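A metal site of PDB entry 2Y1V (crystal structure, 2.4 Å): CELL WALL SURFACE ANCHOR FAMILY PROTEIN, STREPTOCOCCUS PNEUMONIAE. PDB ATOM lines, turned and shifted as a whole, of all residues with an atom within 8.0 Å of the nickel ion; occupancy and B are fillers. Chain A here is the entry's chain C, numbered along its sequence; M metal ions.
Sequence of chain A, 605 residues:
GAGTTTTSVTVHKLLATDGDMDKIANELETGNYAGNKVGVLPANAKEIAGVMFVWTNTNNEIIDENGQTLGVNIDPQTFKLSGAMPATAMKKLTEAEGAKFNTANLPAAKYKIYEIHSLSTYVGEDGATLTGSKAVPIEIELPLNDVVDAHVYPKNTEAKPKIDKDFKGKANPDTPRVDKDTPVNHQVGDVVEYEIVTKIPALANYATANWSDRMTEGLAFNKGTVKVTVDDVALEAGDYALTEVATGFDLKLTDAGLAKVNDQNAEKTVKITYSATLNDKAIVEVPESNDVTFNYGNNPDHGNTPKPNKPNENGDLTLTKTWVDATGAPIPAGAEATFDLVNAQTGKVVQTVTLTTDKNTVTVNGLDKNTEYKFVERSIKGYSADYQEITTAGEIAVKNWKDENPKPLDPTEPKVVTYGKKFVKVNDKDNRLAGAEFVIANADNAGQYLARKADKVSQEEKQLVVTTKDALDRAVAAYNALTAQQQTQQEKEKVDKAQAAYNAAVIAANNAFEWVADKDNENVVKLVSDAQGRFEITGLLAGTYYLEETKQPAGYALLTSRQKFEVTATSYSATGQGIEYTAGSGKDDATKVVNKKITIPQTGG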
ATOM      1  N   LYS A 165       7.769 -27.442  12.438  1.00  0.00           N
ATOM      2  CA  LYS A 165       8.819 -28.282  12.994  1.00  0.00           C
ATOM      3  C   LYS A 165       8.529 -29.754  12.709  1.00  0.00           C
ATOM      4  O   LYS A 165       7.401 -30.222  12.864  1.00  0.00           O
ATOM      5  CB  LYS A 165       9.003 -28.066  14.502  1.00  0.00           C
ATOM      6  CG  LYS A 165       9.924 -29.104  15.126  1.00  0.00           C
ATOM      7  CD  LYS A 165      10.121 -28.907  16.613  1.00  0.00           C
ATOM      8  CE  LYS A 165      10.965 -30.021  17.212  1.00  0.00           C
ATOM      9  NZ  LYS A 165      10.952 -29.963  18.701  1.00  0.00           N
ATOM     10  N   SER A 212      12.143 -21.004  20.583  1.00  0.00           N
ATOM     11  CA  SER A 212      12.283 -21.619  21.886  1.00  0.00           C
ATOM     12  C   SER A 212      11.839 -23.080  21.779  1.00  0.00           C
ATOM     13  O   SER A 212      10.852 -23.395  21.097  1.00  0.00           O
ATOM     14  CB  SER A 212      11.391 -20.868  22.879  1.00  0.00           C
ATOM     15  OG  SER A 212      11.826 -21.034  24.207  1.00  0.00           O
ATOM     16  N   ASP A 213      12.578 -23.981  22.424  1.00  0.00           N
ATOM     17  CA  ASP A 213      12.181 -25.385  22.459  1.00  0.00           C
ATOM     18  C   ASP A 213      12.462 -26.043  23.820  1.00  0.00           C
ATOM     19  O   ASP A 213      13.540 -25.873  24.391  1.00  0.00           O
ATOM     20  CB  ASP A 213      12.826 -26.194  21.313  1.00  0.00           C
ATOM     21  CG  ASP A 213      12.210 -27.593  21.151  1.00  0.00           C
ATOM     22  OD1 ASP A 213      11.166 -27.861  21.792  1.00  0.00           O
ATOM     23  OD2 ASP A 213      12.761 -28.426  20.389  1.00  0.00           O
ATOM     24  N   ARG A 214      11.455 -26.762  24.321  1.00  0.00           N
ATOM     25  CA  ARG A 214      11.515 -27.511  25.569  1.00  0.00           C
ATOM     26  C   ARG A 214      11.036 -28.939  25.294  1.00  0.00           C
ATOM     27  O   ARG A 214      10.105 -29.151  24.502  1.00  0.00           O
ATOM     28  CB  ARG A 214      10.587 -26.884  26.615  1.00  0.00           C
ATOM     29  CG  ARG A 214      11.057 -25.556  27.169  1.00  0.00           C
ATOM     30  CD  ARG A 214      12.440 -25.703  27.745  1.00  0.00           C
ATOM     31  NE  ARG A 214      12.941 -24.508  28.413  1.00  0.00           N
ATOM     32  CZ  ARG A 214      13.501 -23.464  27.795  1.00  0.00           C
ATOM     33  NH1 ARG A 214      13.589 -23.444  26.463  1.00  0.00           N
ATOM     34  NH2 ARG A 214      13.959 -22.434  28.502  1.00  0.00           N
ATOM     35  N   SER A 289       8.374 -35.894  23.221  1.00  0.00           N
ATOM     36  CA  SER A 289       8.177 -34.793  22.274  1.00  0.00           C
ATOM     37  C   SER A 289       8.953 -33.530  22.602  1.00  0.00           C
ATOM     38  O   SER A 289       9.272 -33.245  23.769  1.00  0.00           O
ATOM     39  CB  SER A 289       6.676 -34.452  22.164  1.00  0.00           C
ATOM     40  OG  SER A 289       6.429 -33.450  21.180  1.00  0.00           O
ATOM     41  N   ASN A 290       9.256 -32.774  21.556  1.00  0.00           N
ATOM     42  CA  ASN A 290       9.756 -31.420  21.728  1.00  0.00           C
ATOM     43  C   ASN A 290       8.565 -30.475  21.537  1.00  0.00           C
ATOM     44  O   ASN A 290       7.450 -30.925  21.297  1.00  0.00           O
ATOM     45  CB  ASN A 290      10.866 -31.105  20.739  1.00  0.00           C
ATOM     46  CG  ASN A 290      10.344 -30.965  19.329  1.00  0.00           C
ATOM     47  OD1 ASN A 290       9.456 -31.707  18.923  1.00  0.00           O
ATOM     48  N   ASP A 291       8.805 -29.180  21.633  1.00  0.00           N
ATOM     49  CA  ASP A 291       7.744 -28.194  21.545  1.00  0.00           C
ATOM     50  C   ASP A 291       8.351 -26.822  21.366  1.00  0.00           C
ATOM     51  O   ASP A 291       8.800 -26.201  22.325  1.00  0.00           O
ATOM     52  CB  ASP A 291       6.858 -28.229  22.802  1.00  0.00           C
ATOM     53  CG  ASP A 291       5.601 -27.368  22.668  1.00  0.00           C
ATOM     54  OD1 ASP A 291       5.333 -26.829  21.563  1.00  0.00           O
ATOM     55  OD2 ASP A 291       4.864 -27.241  23.665  1.00  0.00           O
ATOM     56  N   VAL A 292       8.350 -26.358  20.126  1.00  0.00           N
ATOM     57  CA  VAL A 292       8.842 -25.044  19.774  1.00  0.00           C
ATOM     58  C   VAL A 292       7.695 -24.049  19.635  1.00  0.00           C
ATOM     59  O   VAL A 292       6.603 -24.393  19.202  1.00  0.00           O
ATOM     60  CB  VAL A 292       9.589 -25.083  18.420  1.00  0.00           C
ATOM     61  CG1 VAL A 292       9.965 -23.668  17.960  1.00  0.00           C
ATOM     62  CG2 VAL A 292      10.825 -25.946  18.529  1.00  0.00           C
ATOM     63  N   THR A 293       7.959 -22.807  20.033  1.00  0.00           N
ATOM     64  CA  THR A 293       7.149 -21.672  19.648  1.00  0.00           C
ATOM     65  C   THR A 293       8.099 -20.592  19.112  1.00  0.00           C
ATOM     66  O   THR A 293       9.292 -20.595  19.422  1.00  0.00           O
ATOM     67  CB  THR A 293       6.290 -21.146  20.821  1.00  0.00           C
ATOM     68  OG1 THR A 293       7.124 -20.718  21.892  1.00  0.00           O
ATOM     69  CG2 THR A 293       5.358 -22.248  21.324  1.00  0.00           C
ATOM     70  N   PHE A 294       7.576 -19.696  18.283  1.00  0.00           N
ATOM     71  CA  PHE A 294       8.356 -18.605  17.752  1.00  0.00           C
ATOM     72  C   PHE A 294       7.684 -17.340  18.234  1.00  0.00           C
ATOM     73  O   PHE A 294       6.521 -17.110  17.954  1.00  0.00           O
ATOM     74  CB  PHE A 294       8.362 -18.671  16.223  1.00  0.00           C
ATOM     75  CG  PHE A 294       9.057 -17.519  15.556  1.00  0.00           C
ATOM     76  CD1 PHE A 294      10.437 -17.358  15.649  1.00  0.00           C
ATOM     77  CD2 PHE A 294       8.338 -16.607  14.802  1.00  0.00           C
ATOM     78  CE1 PHE A 294      11.077 -16.299  15.014  1.00  0.00           C
ATOM     79  CE2 PHE A 294       8.978 -15.548  14.167  1.00  0.00           C
ATOM     80  CZ  PHE A 294      10.351 -15.396  14.268  1.00  0.00           C
ATOM     81  N   THR A 305       8.338 -20.506  24.934  1.00  0.00           N
ATOM     82  CA  THR A 305       7.618 -21.766  24.772  1.00  0.00           C
ATOM     83  C   THR A 305       7.322 -22.445  26.122  1.00  0.00           C
ATOM     84  O   THR A 305       8.085 -22.280  27.090  1.00  0.00           O
ATOM     85  CB  THR A 305       8.421 -22.712  23.841  1.00  0.00           C
ATOM     86  OG1 THR A 305       7.550 -23.683  23.230  1.00  0.00           O
ATOM     87  CG2 THR A 305       9.568 -23.387  24.596  1.00  0.00           C
ATOM     88  N   PRO A 306       6.209 -23.185  26.202  1.00  0.00           N
ATOM     89  CA  PRO A 306       5.793 -23.798  27.464  1.00  0.00           C
ATOM     90  C   PRO A 306       6.728 -24.897  27.993  1.00  0.00           C
ATOM     91  O   PRO A 306       7.168 -25.770  27.226  1.00  0.00           O
ATOM     92  CB  PRO A 306       4.415 -24.388  27.141  1.00  0.00           C
ATOM     93  CG  PRO A 306       4.362 -24.435  25.650  1.00  0.00           C
ATOM     94  CD  PRO A 306       5.133 -23.255  25.200  1.00  0.00           C
ATOM     95  N   LYS A 374       1.263 -29.624  30.001  1.00  0.00           N
ATOM     96  CA  LYS A 374       1.580 -28.205  29.849  1.00  0.00           C
ATOM     97  C   LYS A 374       0.313 -27.367  29.718  1.00  0.00           C
ATOM     98  O   LYS A 374      -0.650 -27.792  29.104  1.00  0.00           O
ATOM     99  CB  LYS A 374       2.506 -27.986  28.651  1.00  0.00           C
ATOM    100  CG  LYS A 374       1.958 -28.586  27.366  1.00  0.00           C
ATOM    101  CD  LYS A 374       2.947 -28.518  26.203  1.00  0.00           C
ATOM    102  CE  LYS A 374       2.343 -29.116  24.941  1.00  0.00           C
ATOM    103  NZ  LYS A 374       3.190 -28.943  23.739  1.00  0.00           N
ATOM    104  N   VAL A 376      -1.040 -24.455  27.853  1.00  0.00           N
ATOM    105  CA  VAL A 376      -0.779 -23.640  26.700  1.00  0.00           C
ATOM    106  C   VAL A 376      -1.803 -22.505  26.667  1.00  0.00           C
ATOM    107  O   VAL A 376      -3.011 -22.735  26.739  1.00  0.00           O
ATOM    108  CB  VAL A 376      -0.877 -24.469  25.399  1.00  0.00           C
ATOM    109  CG1 VAL A 376      -0.607 -23.604  24.182  1.00  0.00           C
ATOM    110  CG2 VAL A 376       0.073 -25.624  25.461  1.00  0.00           C
ATOM    111  N   LEU A 409       3.850 -17.838  16.848  1.00  0.00           N
ATOM    112  CA  LEU A 409       3.646 -18.949  15.920  1.00  0.00           C
ATOM    113  C   LEU A 409       3.887 -20.249  16.672  1.00  0.00           C
ATOM    114  O   LEU A 409       4.854 -20.338  17.442  1.00  0.00           O
ATOM    115  CB  LEU A 409       4.587 -18.851  14.715  1.00  0.00           C
ATOM    116  CG  LEU A 409       4.148 -17.919  13.584  1.00  0.00           C
ATOM    117  CD1 LEU A 409       4.713 -18.407  12.242  1.00  0.00           C
ATOM    118  CD2 LEU A 409       2.629 -17.842  13.504  1.00  0.00           C
ATOM    119  N   ASP A 410       3.023 -21.247  16.478  1.00  0.00           N
ATOM    120  CA  ASP A 410       3.109 -22.465  17.266  1.00  0.00           C
ATOM    121  C   ASP A 410       2.825 -23.737  16.475  1.00  0.00           C
ATOM    122  O   ASP A 410       1.747 -24.310  16.601  1.00  0.00           O
ATOM    123  CB  ASP A 410       2.194 -22.395  18.496  1.00  0.00           C
ATOM    124  CG  ASP A 410       2.549 -23.434  19.561  1.00  0.00           C
ATOM    125  OD1 ASP A 410       3.673 -24.002  19.476  1.00  0.00           O
ATOM    126  OD2 ASP A 410       1.726 -23.660  20.481  1.00  0.00           O
ATOM    127  N   PRO A 411       3.811 -24.198  15.693  1.00  0.00           N
ATOM    128  CA  PRO A 411       3.686 -25.377  14.860  1.00  0.00           C
ATOM    129  C   PRO A 411       3.464 -26.611  15.715  1.00  0.00           C
ATOM    130  O   PRO A 411       3.754 -26.580  16.912  1.00  0.00           O
ATOM    131  CB  PRO A 411       5.052 -25.471  14.215  1.00  0.00           C
ATOM    132  CG  PRO A 411       5.971 -24.948  15.275  1.00  0.00           C
ATOM    133  CD  PRO A 411       5.217 -23.784  15.829  1.00  0.00           C
ATOM    134  N   THR A 412       2.955 -27.686  15.124  1.00  0.00           N
ATOM    135  CA  THR A 412       2.842 -28.970  15.826  1.00  0.00           C
ATOM    136  C   THR A 412       4.203 -29.665  15.776  1.00  0.00           C
ATOM    137  O   THR A 412       5.062 -29.299  14.962  1.00  0.00           O
ATOM    138  CB  THR A 412       1.821 -29.888  15.158  1.00  0.00           C
ATOM    139  OG1 THR A 412       1.892 -29.686  13.743  1.00  0.00           O
ATOM    140  CG2 THR A 412       0.398 -29.595  15.646  1.00  0.00           C
ATOM    141  N   GLU A 413       4.385 -30.678  16.626  1.00  0.00           N
ATOM    142  CA  GLU A 413       5.641 -31.393  16.665  1.00  0.00           C
ATOM    143  C   GLU A 413       5.484 -32.913  16.502  1.00  0.00           C
ATOM    144  O   GLU A 413       4.442 -33.474  16.822  1.00  0.00           O
ATOM    145  CB  GLU A 413       6.414 -31.030  17.937  1.00  0.00           C
ATOM    146  CG  GLU A 413       6.885 -29.573  17.975  1.00  0.00           C
ATOM    147  CD  GLU A 413       6.078 -28.684  18.901  1.00  0.00           C
ATOM    148  OE1 GLU A 413       5.173 -29.210  19.586  1.00  0.00           O
ATOM    149  OE2 GLU A 413       6.354 -27.457  18.955  1.00  0.00           O
ATOM    150  N   LYS A 415       6.575 -37.107  16.988  1.00  0.00           N
ATOM    151  CA  LYS A 415       6.673 -37.866  18.225  1.00  0.00           C
ATOM    152  C   LYS A 415       7.513 -39.128  18.052  1.00  0.00           C
ATOM    153  O   LYS A 415       7.621 -39.678  16.945  1.00  0.00           O
ATOM    154  CB  LYS A 415       5.280 -38.220  18.757  1.00  0.00           C
ATOM    155  CG  LYS A 415       4.307 -37.036  18.820  1.00  0.00           C
ATOM    156  CD  LYS A 415       4.404 -36.325  20.156  1.00  0.00           C
ATOM    157  CE  LYS A 415       3.604 -35.021  20.184  1.00  0.00           C
ATOM    158  NZ  LYS A 415       4.380 -33.849  19.664  1.00  0.00           N
HETATM  159 NI    NI M   1       4.606 -26.056  19.702  1.00  0.00          NI
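The side-chain carboxylate of Asp 291 lies close to the side-chain amino group of Lys 374, at 3.7 Å.
The side-chain hydroxyl (OG1) of Thr 305 is in hydrogen-bond range of the backbone carbonyl oxygen (O) of Asp 291 (3.0 Å).
N of Asp 291 is in hydrogen-bond range of OD1 of Asp 213 (2.7 Å).
The backbone carbonyl oxygen (O) of Arg 214 sits at hydrogen-bond distance from the backbone NH (N) of Asp 291 (3.1 Å).
The side-chain carboxylate (OE2) of Glu 413 sits close to the backbone NH (N) of Val 292 (2.6 Å).
O of Glu 413 lies within hydrogen-bond range of NZ of Lys 415 (2.9 Å).
Merely in contact with the nickel ion: Pro 411 (3.0 Å).
Five residues have an atom within 4 Å of the nickel ion: Asp 291, Val 292, Asp 410, Pro 411 and Glu 413.
The nearest printed residue that does not touch the nickel ion is Thr 293 (4.2 Å).
OD1 of Asp 291 is bound to the nickel ion (2.1 Å).
The nickel ion is bound by the side-chain carboxylate (OD1) of Asp 410.
OE2 of Glu 413 binds the nickel ion, 2.4 Å away.
Slightly farther from the nickel ion lies the backbone carbonyl oxygen (O) of Val 292 (2.6 Å).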
